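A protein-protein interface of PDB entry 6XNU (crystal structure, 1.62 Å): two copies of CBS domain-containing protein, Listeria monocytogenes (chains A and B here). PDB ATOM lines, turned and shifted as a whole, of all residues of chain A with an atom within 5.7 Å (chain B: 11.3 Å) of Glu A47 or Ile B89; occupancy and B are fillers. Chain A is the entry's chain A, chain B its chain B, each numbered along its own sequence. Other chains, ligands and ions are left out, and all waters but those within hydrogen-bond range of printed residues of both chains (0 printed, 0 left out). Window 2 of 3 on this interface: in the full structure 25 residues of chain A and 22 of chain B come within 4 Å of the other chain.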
ATOM      1  N   ASN A  45     -18.297   3.375   6.742  1.00  0.00           N
ATOM      2  CA  ASN A  45     -17.876   2.946   8.064  1.00  0.00           C
ATOM      3  C   ASN A  45     -18.188   4.033   9.093  1.00  0.00           C
ATOM      4  O   ASN A  45     -18.606   5.147   8.757  1.00  0.00           O
ATOM      5  CB  ASN A  45     -16.388   2.555   8.078  1.00  0.00           C
ATOM      6  CG  ASN A  45     -15.453   3.723   7.833  1.00  0.00           C
ATOM      7  OD1 ASN A  45     -15.539   4.764   8.479  1.00  0.00           O
ATOM      8  ND2 ASN A  45     -14.510   3.531   6.915  1.00  0.00           N
ATOM      9  N   LEU A  46     -18.007   3.681  10.370  1.00  0.00           N
ATOM     10  CA  LEU A  46     -18.390   4.583  11.459  1.00  0.00           C
ATOM     11  C   LEU A  46     -17.417   5.739  11.642  1.00  0.00           C
ATOM     12  O   LEU A  46     -17.802   6.786  12.174  1.00  0.00           O
ATOM     13  CB  LEU A  46     -18.521   3.810  12.771  1.00  0.00           C
ATOM     14  CG  LEU A  46     -19.551   2.681  12.798  1.00  0.00           C
ATOM     15  CD1 LEU A  46     -19.773   2.220  14.227  1.00  0.00           C
ATOM     16  CD2 LEU A  46     -20.871   3.101  12.149  1.00  0.00           C
ATOM     17  N   GLU A  47     -16.156   5.572  11.239  1.00  0.00           N
ATOM     18  CA  GLU A  47     -15.239   6.706  11.269  1.00  0.00           C
ATOM     19  C   GLU A  47     -15.692   7.789  10.296  1.00  0.00           C
ATOM     20  O   GLU A  47     -15.714   8.977  10.643  1.00  0.00           O
ATOM     21  CB  GLU A  47     -13.809   6.245  10.965  1.00  0.00           C
ATOM     22  CG  GLU A  47     -12.835   7.393  10.685  1.00  0.00           C
ATOM     23  CD  GLU A  47     -11.559   7.324  11.511  1.00  0.00           C
ATOM     24  OE1 GLU A  47     -11.184   6.213  11.944  1.00  0.00           O
ATOM     25  OE2 GLU A  47     -10.926   8.386  11.721  1.00  0.00           O
ATOM     26  N   HIS A  48     -16.105   7.392   9.087  1.00  0.00           N
ATOM     27  CA  HIS A  48     -16.636   8.365   8.138  1.00  0.00           C
ATOM     28  C   HIS A  48     -17.892   9.037   8.686  1.00  0.00           C
ATOM     29  O   HIS A  48     -18.036  10.264   8.606  1.00  0.00           O
ATOM     30  CB  HIS A  48     -16.933   7.687   6.800  1.00  0.00           C
ATOM     31  CG  HIS A  48     -17.458   8.625   5.758  1.00  0.00           C
ATOM     32  ND1 HIS A  48     -18.783   8.655   5.379  1.00  0.00           N
ATOM     33  CD2 HIS A  48     -16.838   9.589   5.036  1.00  0.00           C
ATOM     34  CE1 HIS A  48     -18.955   9.586   4.458  1.00  0.00           C
ATOM     35  NE2 HIS A  48     -17.789  10.163   4.229  1.00  0.00           N
ATOM     36  N   ALA A  49     -18.801   8.251   9.268  1.00  0.00           N
ATOM     37  CA  ALA A  49     -20.030   8.822   9.819  1.00  0.00           C
ATOM     38  C   ALA A  49     -19.734   9.829  10.924  1.00  0.00           C
ATOM     39  O   ALA A  49     -20.402  10.867  11.028  1.00  0.00           O
ATOM     40  CB  ALA A  49     -20.938   7.710  10.341  1.00  0.00           C
ATOM     41  N   LEU A  50     -18.742   9.536  11.771  1.00  0.00           N
ATOM     42  CA  LEU A  50     -18.401  10.458  12.847  1.00  0.00           C
ATOM     43  C   LEU A  50     -17.915  11.789  12.289  1.00  0.00           C
ATOM     44  O   LEU A  50     -18.238  12.860  12.823  1.00  0.00           O
ATOM     45  CB  LEU A  50     -17.336   9.819  13.746  1.00  0.00           C
ATOM     46  CG  LEU A  50     -17.456   9.932  15.260  1.00  0.00           C
ATOM     47  CD1 LEU A  50     -18.870   9.646  15.776  1.00  0.00           C
ATOM     48  CD2 LEU A  50     -16.439   8.977  15.893  1.00  0.00           C
ATOM     49  N   LEU A  51     -17.143  11.737  11.205  1.00  0.00           N
ATOM     50  CA  LEU A  51     -16.678  12.958  10.561  1.00  0.00           C
ATOM     51  C   LEU A  51     -17.849  13.769  10.024  1.00  0.00           C
ATOM     52  O   LEU A  51     -17.945  14.975  10.270  1.00  0.00           O
ATOM     53  CB  LEU A  51     -15.700  12.609   9.444  1.00  0.00           C
ATOM     54  CG  LEU A  51     -15.232  13.721   8.512  1.00  0.00           C
ATOM     55  CD1 LEU A  51     -14.367  14.713   9.271  1.00  0.00           C
ATOM     56  CD2 LEU A  51     -14.465  13.110   7.344  1.00  0.00           C
ATOM     57  N   VAL A  52     -18.762  13.115   9.298  1.00  0.00           N
ATOM     58  CA  VAL A  52     -19.917  13.827   8.756  1.00  0.00           C
ATOM     59  C   VAL A  52     -20.735  14.448   9.879  1.00  0.00           C
ATOM     60  O   VAL A  52     -21.126  15.620   9.818  1.00  0.00           O
ATOM     61  CB  VAL A  52     -20.778  12.886   7.891  1.00  0.00           C
ATOM     62  CG1 VAL A  52     -22.063  13.606   7.479  1.00  0.00           C
ATOM     63  CG2 VAL A  52     -20.002  12.418   6.682  1.00  0.00           C
ATOM     64  N   PHE A  91     -11.813   2.945  19.751  1.00  0.00           N
ATOM     65  CA  PHE A  91     -11.876   3.768  18.547  1.00  0.00           C
ATOM     66  C   PHE A  91     -11.295   3.067  17.323  1.00  0.00           C
ATOM     67  O   PHE A  91     -11.660   3.413  16.195  1.00  0.00           O
ATOM     68  CB  PHE A  91     -11.145   5.093  18.775  1.00  0.00           C
ATOM     69  CG  PHE A  91     -11.722   5.925  19.890  1.00  0.00           C
ATOM     70  CD1 PHE A  91     -12.963   6.524  19.752  1.00  0.00           C
ATOM     71  CD2 PHE A  91     -11.023   6.104  21.073  1.00  0.00           C
ATOM     72  CE1 PHE A  91     -13.494   7.292  20.771  1.00  0.00           C
ATOM     73  CE2 PHE A  91     -11.548   6.866  22.099  1.00  0.00           C
ATOM     74  CZ  PHE A  91     -12.785   7.458  21.951  1.00  0.00           C
ATOM     75  N   LEU A  94     -13.847   1.633  14.738  1.00  0.00           N
ATOM     76  CA  LEU A  94     -14.709   2.470  13.903  1.00  0.00           C
ATOM     77  C   LEU A  94     -14.467   2.197  12.427  1.00  0.00           C
ATOM     78  O   LEU A  94     -15.400   2.236  11.616  1.00  0.00           O
ATOM     79  CB  LEU A  94     -14.468   3.947  14.209  1.00  0.00           C
ATOM     80  CG  LEU A  94     -14.806   4.369  15.630  1.00  0.00           C
ATOM     81  CD1 LEU A  94     -14.223   5.734  15.924  1.00  0.00           C
ATOM     82  CD2 LEU A  94     -16.315   4.381  15.797  1.00  0.00           C
ATOM     83  N   GLU A  95     -13.213   1.912  12.068  1.00  0.00           N
ATOM     84  CA  GLU A  95     -12.859   1.601  10.689  1.00  0.00           C
ATOM     85  C   GLU A  95     -13.627   0.404  10.155  1.00  0.00           C
ATOM     86  O   GLU A  95     -13.905   0.333   8.952  1.00  0.00           O
ATOM     87  CB  GLU A  95     -11.355   1.342  10.616  1.00  0.00           C
ATOM     88  CG  GLU A  95     -10.752   1.242   9.232  1.00  0.00           C
ATOM     89  CD  GLU A  95      -9.245   1.069   9.303  1.00  0.00           C
ATOM     90  OE1 GLU A  95      -8.617   1.741  10.154  1.00  0.00           O
ATOM     91  OE2 GLU A  95      -8.691   0.256   8.529  1.00  0.00           O
ATOM     92  N   LEU A  97     -16.679  -1.191  11.455  1.00  0.00           N
ATOM     93  CA  LEU A  97     -18.125  -1.278  11.565  1.00  0.00           C
ATOM     94  C   LEU A  97     -18.774  -0.369  10.525  1.00  0.00           C
ATOM     95  O   LEU A  97     -18.197   0.647  10.127  1.00  0.00           O
ATOM     96  CB  LEU A  97     -18.583  -0.885  12.971  1.00  0.00           C
ATOM     97  CG  LEU A  97     -18.140  -1.812  14.106  1.00  0.00           C
ATOM     98  CD1 LEU A  97     -17.846  -1.015  15.371  1.00  0.00           C
ATOM     99  CD2 LEU A  97     -19.222  -2.850  14.359  1.00  0.00           C
ATOM    100  N   LEU B  46     -11.708  14.717  27.905  1.00  0.00           N
ATOM    101  CA  LEU B  46     -12.748  14.527  26.894  1.00  0.00           C
ATOM    102  C   LEU B  46     -13.136  13.068  26.749  1.00  0.00           C
ATOM    103  O   LEU B  46     -14.241  12.775  26.282  1.00  0.00           O
ATOM    104  CB  LEU B  46     -12.299  15.078  25.535  1.00  0.00           C
ATOM    105  CG  LEU B  46     -11.890  16.550  25.516  1.00  0.00           C
ATOM    106  CD1 LEU B  46     -11.699  16.992  24.074  1.00  0.00           C
ATOM    107  CD2 LEU B  46     -12.914  17.439  26.246  1.00  0.00           C
ATOM    108  N   LEU B  50     -16.995  11.983  26.785  1.00  0.00           N
ATOM    109  CA  LEU B  50     -17.603  11.154  25.742  1.00  0.00           C
ATOM    110  C   LEU B  50     -18.338   9.963  26.342  1.00  0.00           C
ATOM    111  O   LEU B  50     -19.411   9.576  25.863  1.00  0.00           O
ATOM    112  CB  LEU B  50     -16.533  10.673  24.760  1.00  0.00           C
ATOM    113  CG  LEU B  50     -16.229  11.532  23.537  1.00  0.00           C
ATOM    114  CD1 LEU B  50     -15.315  10.757  22.588  1.00  0.00           C
ATOM    115  CD2 LEU B  50     -17.503  11.976  22.806  1.00  0.00           C
ATOM    116  N   ALA B  76     -20.729  15.871  21.895  1.00  0.00           N
ATOM    117  CA  ALA B  76     -19.772  15.032  21.172  1.00  0.00           C
ATOM    118  C   ALA B  76     -19.191  15.758  19.962  1.00  0.00           C
ATOM    119  O   ALA B  76     -18.023  15.542  19.615  1.00  0.00           O
ATOM    120  CB  ALA B  76     -20.424  13.717  20.740  1.00  0.00           C
ATOM    121  N   ALA B  77     -19.977  16.626  19.311  1.00  0.00           N
ATOM    122  CA  ALA B  77     -19.456  17.330  18.141  1.00  0.00           C
ATOM    123  C   ALA B  77     -18.361  18.318  18.529  1.00  0.00           C
ATOM    124  O   ALA B  77     -17.359  18.445  17.814  1.00  0.00           O
ATOM    125  CB  ALA B  77     -20.589  18.046  17.406  1.00  0.00           C
ATOM    126  N   MET B  78     -18.531  19.021  19.655  1.00  0.00           N
ATOM    127  CA  MET B  78     -17.467  19.892  20.148  1.00  0.00           C
ATOM    128  C   MET B  78     -16.208  19.094  20.451  1.00  0.00           C
ATOM    129  O   MET B  78     -15.083  19.532  20.157  1.00  0.00           O
ATOM    130  CB  MET B  78     -17.925  20.620  21.414  1.00  0.00           C
ATOM    131  CG  MET B  78     -19.141  21.495  21.245  1.00  0.00           C
ATOM    132  SD  MET B  78     -19.564  22.204  22.835  1.00  0.00           S
ATOM    133  CE  MET B  78     -21.278  22.621  22.534  1.00  0.00           C
ATOM    134  N   ILE B  79     -16.380  17.923  21.057  1.00  0.00           N
ATOM    135  CA  ILE B  79     -15.234  17.099  21.433  1.00  0.00           C
ATOM    136  C   ILE B  79     -14.514  16.590  20.193  1.00  0.00           C
ATOM    137  O   ILE B  79     -13.276  16.631  20.110  1.00  0.00           O
ATOM    138  CB  ILE B  79     -15.708  15.946  22.336  1.00  0.00           C
ATOM    139  CG1 ILE B  79     -16.100  16.476  23.717  1.00  0.00           C
ATOM    140  CG2 ILE B  79     -14.644  14.842  22.436  1.00  0.00           C
ATOM    141  CD1 ILE B  79     -16.809  15.444  24.558  1.00  0.00           C
ATOM    142  N   THR B  80     -15.273  16.098  19.211  1.00  0.00           N
ATOM    143  CA  THR B  80     -14.645  15.505  18.041  1.00  0.00           C
ATOM    144  C   THR B  80     -14.041  16.563  17.131  1.00  0.00           C
ATOM    145  O   THR B  80     -12.984  16.332  16.533  1.00  0.00           O
ATOM    146  CB  THR B  80     -15.665  14.646  17.297  1.00  0.00           C
ATOM    147  OG1 THR B  80     -16.209  13.687  18.216  1.00  0.00           O
ATOM    148  CG2 THR B  80     -14.997  13.907  16.144  1.00  0.00           C
ATOM    149  N   ASP B  81     -14.682  17.730  17.021  1.00  0.00           N
ATOM    150  CA  ASP B  81     -14.081  18.820  16.263  1.00  0.00           C
ATOM    151  C   ASP B  81     -12.712  19.184  16.820  1.00  0.00           C
ATOM    152  O   ASP B  81     -11.793  19.508  16.062  1.00  0.00           O
ATOM    153  CB  ASP B  81     -14.998  20.039  16.274  1.00  0.00           C
ATOM    154  CG  ASP B  81     -14.304  21.287  15.770  1.00  0.00           C
ATOM    155  OD1 ASP B  81     -14.198  21.438  14.535  1.00  0.00           O
ATOM    156  OD2 ASP B  81     -13.841  22.104  16.603  1.00  0.00           O
ATOM    157  N   ALA B  82     -12.556  19.125  18.143  1.00  0.00           N
ATOM    158  CA  ALA B  82     -11.297  19.530  18.752  1.00  0.00           C
ATOM    159  C   ALA B  82     -10.151  18.591  18.405  1.00  0.00           C
ATOM    160  O   ALA B  82      -8.986  18.999  18.495  1.00  0.00           O
ATOM    161  CB  ALA B  82     -11.454  19.619  20.270  1.00  0.00           C
ATOM    162  N   ILE B  83     -10.440  17.351  18.018  1.00  0.00           N
ATOM    163  CA  ILE B  83      -9.401  16.369  17.720  1.00  0.00           C
ATOM    164  C   ILE B  83      -9.360  16.015  16.240  1.00  0.00           C
ATOM    165  O   ILE B  83      -8.714  15.034  15.859  1.00  0.00           O
ATOM    166  CB  ILE B  83      -9.556  15.104  18.582  1.00  0.00           C
ATOM    167  CG1 ILE B  83     -10.909  14.432  18.322  1.00  0.00           C
ATOM    168  CG2 ILE B  83      -9.387  15.441  20.061  1.00  0.00           C
ATOM    169  CD1 ILE B  83     -10.966  12.982  18.785  1.00  0.00           C
ATOM    170  N   LEU B  84     -10.043  16.783  15.392  1.00  0.00           N
ATOM    171  CA  LEU B  84      -9.957  16.582  13.947  1.00  0.00           C
ATOM    172  C   LEU B  84      -8.601  17.070  13.448  1.00  0.00           C
ATOM    173  O   LEU B  84      -8.324  18.274  13.470  1.00  0.00           O
ATOM    174  CB  LEU B  84     -11.085  17.327  13.239  1.00  0.00           C
ATOM    175  CG  LEU B  84     -12.473  16.689  13.219  1.00  0.00           C
ATOM    176  CD1 LEU B  84     -13.284  17.216  12.047  1.00  0.00           C
ATOM    177  CD2 LEU B  84     -12.363  15.181  13.150  1.00  0.00           C
ATOM    178  N   GLY B  85      -7.750  16.144  12.999  1.00  0.00           N
ATOM    179  CA  GLY B  85      -6.511  16.510  12.348  1.00  0.00           C
ATOM    180  C   GLY B  85      -6.703  16.770  10.862  1.00  0.00           C
ATOM    181  O   GLY B  85      -7.791  16.637  10.305  1.00  0.00           O
ATOM    182  N   LEU B  86      -5.611  17.171  10.214  1.00  0.00           N
ATOM    183  CA  LEU B  86      -5.629  17.349   8.768  1.00  0.00           C
ATOM    184  C   LEU B  86      -5.609  16.021   8.022  1.00  0.00           C
ATOM    185  O   LEU B  86      -5.908  15.993   6.825  1.00  0.00           O
ATOM    186  CB  LEU B  86      -4.443  18.215   8.325  1.00  0.00           C
ATOM    187  CG  LEU B  86      -4.472  19.671   8.801  1.00  0.00           C
ATOM    188  CD1 LEU B  86      -3.145  20.355   8.555  1.00  0.00           C
ATOM    189  CD2 LEU B  86      -5.611  20.443   8.131  1.00  0.00           C
ATOM    190  N   GLU B  87      -5.267  14.924   8.705  1.00  0.00           N
ATOM    191  CA  GLU B  87      -5.233  13.597   8.103  1.00  0.00           C
ATOM    192  C   GLU B  87      -6.089  12.567   8.825  1.00  0.00           C
ATOM    193  O   GLU B  87      -6.480  11.574   8.200  1.00  0.00           O
ATOM    194  CB  GLU B  87      -3.789  13.074   8.056  1.00  0.00           C
ATOM    195  CG  GLU B  87      -3.105  13.137   9.414  1.00  0.00           C
ATOM    196  CD  GLU B  87      -1.697  12.583   9.403  1.00  0.00           C
ATOM    197  OE1 GLU B  87      -1.301  11.963   8.389  1.00  0.00           O
ATOM    198  OE2 GLU B  87      -0.990  12.769  10.419  1.00  0.00           O
ATOM    199  N   ARG B  88      -6.407  12.775  10.101  1.00  0.00           N
ATOM    200  CA  ARG B  88      -7.019  11.737  10.918  1.00  0.00           C
ATOM    201  C   ARG B  88      -7.811  12.377  12.049  1.00  0.00           C
ATOM    202  O   ARG B  88      -7.577  13.532  12.416  1.00  0.00           O
ATOM    203  CB  ARG B  88      -5.949  10.801  11.483  1.00  0.00           C
ATOM    204  CG  ARG B  88      -6.288   9.335  11.429  1.00  0.00           C
ATOM    205  CD  ARG B  88      -5.282   8.531  12.235  1.00  0.00           C
ATOM    206  NE  ARG B  88      -5.090   9.054  13.587  1.00  0.00           N
ATOM    207  CZ  ARG B  88      -3.993   9.688  13.997  1.00  0.00           C
ATOM    208  NH1 ARG B  88      -3.900  10.123  15.249  1.00  0.00           N
ATOM    209  NH2 ARG B  88      -2.995   9.900  13.151  1.00  0.00           N
ATOM    210  N   ILE B  89      -8.759  11.615  12.593  1.00  0.00           N
ATOM    211  CA  ILE B  89      -9.384  11.959  13.870  1.00  0.00           C
ATOM    212  C   ILE B  89      -8.458  11.449  14.966  1.00  0.00           C
ATOM    213  O   ILE B  89      -8.290  10.239  15.131  1.00  0.00           O
ATOM    214  CB  ILE B  89     -10.783  11.352  14.020  1.00  0.00           C
ATOM    215  CG1 ILE B  89     -11.709  11.780  12.879  1.00  0.00           C
ATOM    216  CG2 ILE B  89     -11.377  11.763  15.356  1.00  0.00           C
ATOM    217  CD1 ILE B  89     -13.170  11.422  13.118  1.00  0.00           C
ATOM    218  N   GLU B  90      -7.859  12.368  15.722  1.00  0.00           N
ATOM    219  CA  GLU B  90      -6.747  12.025  16.609  1.00  0.00           C
ATOM    220  C   GLU B  90      -7.283  11.685  17.999  1.00  0.00           C
ATOM    221  O   GLU B  90      -7.196  12.465  18.950  1.00  0.00           O
ATOM    222  CB  GLU B  90      -5.733  13.161  16.632  1.00  0.00           C
ATOM    223  CG  GLU B  90      -5.146  13.432  15.246  1.00  0.00           C
ATOM    224  CD  GLU B  90      -4.460  14.778  15.116  1.00  0.00           C
ATOM    225  OE1 GLU B  90      -4.270  15.468  16.138  1.00  0.00           O
ATOM    226  OE2 GLU B  90      -4.101  15.144  13.976  1.00  0.00           O
ATOM    227  N   PHE B  91      -7.825  10.467  18.109  1.00  0.00           N
ATOM    228  CA  PHE B  91      -8.498  10.040  19.336  1.00  0.00           C
ATOM    229  C   PHE B  91      -7.555  10.020  20.531  1.00  0.00           C
ATOM    230  O   PHE B  91      -7.998  10.194  21.671  1.00  0.00           O
ATOM    231  CB  PHE B  91      -9.130   8.659  19.140  1.00  0.00           C
ATOM    232  CG  PHE B  91     -10.259   8.645  18.150  1.00  0.00           C
ATOM    233  CD1 PHE B  91     -11.485   9.207  18.474  1.00  0.00           C
ATOM    234  CD2 PHE B  91     -10.098   8.068  16.901  1.00  0.00           C
ATOM    235  CE1 PHE B  91     -12.535   9.200  17.569  1.00  0.00           C
ATOM    236  CE2 PHE B  91     -11.143   8.056  15.987  1.00  0.00           C
ATOM    237  CZ  PHE B  91     -12.363   8.620  16.326  1.00  0.00           C
ATOM    238  N   GLU B  92      -6.257   9.813  20.302  1.00  0.00           N
ATOM    239  CA  GLU B  92      -5.320   9.804  21.419  1.00  0.00           C
ATOM    240  C   GLU B  92      -5.306  11.129  22.179  1.00  0.00           C
ATOM    241  O   GLU B  92      -4.903  11.159  23.348  1.00  0.00           O
ATOM    242  CB  GLU B  92      -3.911   9.453  20.915  1.00  0.00           C
ATOM    243  CG  GLU B  92      -3.242  10.557  20.101  1.00  0.00           C
ATOM    244  CD  GLU B  92      -3.576  10.496  18.614  1.00  0.00           C
ATOM    245  OE1 GLU B  92      -4.335   9.592  18.196  1.00  0.00           O
ATOM    246  OE2 GLU B  92      -3.077  11.358  17.858  1.00  0.00           O
ATOM    247  N   ARG B  93      -5.764  12.220  21.560  1.00  0.00           N
ATOM    248  CA  ARG B  93      -5.753  13.516  22.217  1.00  0.00           C
ATOM    249  C   ARG B  93      -6.929  13.718  23.164  1.00  0.00           C
ATOM    250  O   ARG B  93      -6.966  14.739  23.861  1.00  0.00           O
ATOM    251  CB  ARG B  93      -5.733  14.633  21.170  1.00  0.00           C
ATOM    252  CG  ARG B  93      -4.415  14.744  20.418  1.00  0.00           C
ATOM    253  CD  ARG B  93      -4.522  15.717  19.259  1.00  0.00           C
ATOM    254  NE  ARG B  93      -4.892  17.059  19.702  1.00  0.00           N
ATOM    255  CZ  ARG B  93      -5.516  17.953  18.940  1.00  0.00           C
ATOM    256  NH1 ARG B  93      -5.845  17.654  17.688  1.00  0.00           N
ATOM    257  NH2 ARG B  93      -5.808  19.149  19.430  1.00  0.00           N
ATOM    258  N   LEU B  94      -7.871  12.774  23.227  1.00  0.00           N
ATOM    259  CA  LEU B  94      -9.007  12.939  24.133  1.00  0.00           C
ATOM    260  C   LEU B  94      -8.555  12.980  25.584  1.00  0.00           C
ATOM    261  O   LEU B  94      -9.143  13.691  26.404  1.00  0.00           O
ATOM    262  CB  LEU B  94     -10.010  11.812  23.942  1.00  0.00           C
ATOM    263  CG  LEU B  94     -10.693  11.839  22.587  1.00  0.00           C
ATOM    264  CD1 LEU B  94     -11.414  10.530  22.351  1.00  0.00           C
ATOM    265  CD2 LEU B  94     -11.642  13.021  22.521  1.00  0.00           C
ATOM    266  N   GLU B  95      -7.527  12.205  25.929  1.00  0.00           N
ATOM    267  CA  GLU B  95      -7.051  12.225  27.308  1.00  0.00           C
ATOM    268  C   GLU B  95      -6.212  13.458  27.622  1.00  0.00           C
ATOM    269  O   GLU B  95      -5.994  13.749  28.805  1.00  0.00           O
ATOM    270  CB  GLU B  95      -6.254  10.950  27.612  1.00  0.00           C
ATOM    271  CG  GLU B  95      -4.944  10.851  26.870  1.00  0.00           C
ATOM    272  CD  GLU B  95      -4.195   9.560  27.169  1.00  0.00           C
ATOM    273  OE1 GLU B  95      -4.755   8.679  27.866  1.00  0.00           O
ATOM    274  OE2 GLU B  95      -3.049   9.427  26.696  1.00  0.00           O
ATOM    275  N   LEU B  97      -6.998  16.711  26.480  1.00  0.00           N
ATOM    276  CA  LEU B  97      -7.815  17.915  26.521  1.00  0.00           C
ATOM    277  C   LEU B  97      -8.831  17.807  27.648  1.00  0.00           C
ATOM    278  O   LEU B  97      -9.300  16.712  27.965  1.00  0.00           O
ATOM    279  CB  LEU B  97      -8.544  18.128  25.190  1.00  0.00           C
ATOM    280  CG  LEU B  97      -7.683  18.361  23.948  1.00  0.00           C
ATOM    281  CD1 LEU B  97      -8.362  17.805  22.693  1.00  0.00           C
ATOM    282  CD2 LEU B  97      -7.384  19.834  23.782  1.00  0.00           C
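Phe A91 touches its own counterpart, Phe B91.
Phe A91 touches Leu B94, and with the chains exchanged Leu A94 touches Phe B91.
6 positions are printed for both chains.
Of the 5 pairs that touch across the chains among the printed residues, 3 have their exchanged pair printed and touching as well.
Glu A47 touches Ile B89.
Leu A51 touches Leu B84.
Phe A91 touches Phe B91.
CZ of Phe A91 touches CD1 of Leu B94 (3.4 Å).
CD1 of Leu A94 touches CZ of Phe B91 (3.5 Å).
Of the 23 printed residues of chain B, 4 touch a printed residue of chain A.
Hydrophobic or aromatic side chains of chain B within 4 Å of the printed part of chain A: Leu B84, Ile B89, Phe B91 and Leu B94.
Along chain A the printed residues that touch a printed residue of chain B span positions 47 to 94.
Among the printed residues, no Asp or Glu carboxylate lies within 4 Å of a Lys or Arg side-chain nitrogen of the other chain.
The backbone carbonyl oxygen of Leu A94 lies within hydrogen-bond range of the backbone NH of Glu A47.
The backbone NH (N) of Glu A47 is in hydrogen-bond range of the side-chain amide oxygen (OD1) of Asn A45 (2.9 Å).
The backbone carbonyl oxygen of Leu A94 sits at hydrogen-bond distance from the backbone NH of Leu A46, 3.2 Å away.
N of Leu B46 is in hydrogen-bond range of O of Leu B94 (3.1 Å).
Glu A47 touches just one residue of chain B: Ile B89.
Of the printed residues of chain A, Ile B89 touches Glu A47 (3.7 Å).
No residue of chain B comes within 4 Å of Asn A45.
No residue of chain B comes within 4 Å of Leu A46.
No residue of chain B comes within 4 Å of His A48.
No residue of chain B comes within 4 Å of Ala A49.
No residue of chain B comes within 4 Å of Leu A50.
Of chain B, only Leu B84 comes within 4 Å of Leu A51.
Leu A94 touches one residue of chain B.
Printed residues of chain A within 4 Å of Leu B94: Phe A91.
Of the printed residues of chain A, Leu B84 touches Leu A51.
Printed residues of chain A within 4 Å of Phe B91: Phe A91 (3.3 Å) and Leu A94 (3.5 Å).
Of the printed residues of chain B, Phe A91 touches Phe B91 and Leu B94.
Ala B82 touches none of the printed residues of chain A.
The nearest residue of chain A that does not touch Ile B89 is Leu A51 (4.4 Å).
The nearest printed residue of chain A that does not touch Phe B91 is Leu A50 (4.1 Å).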
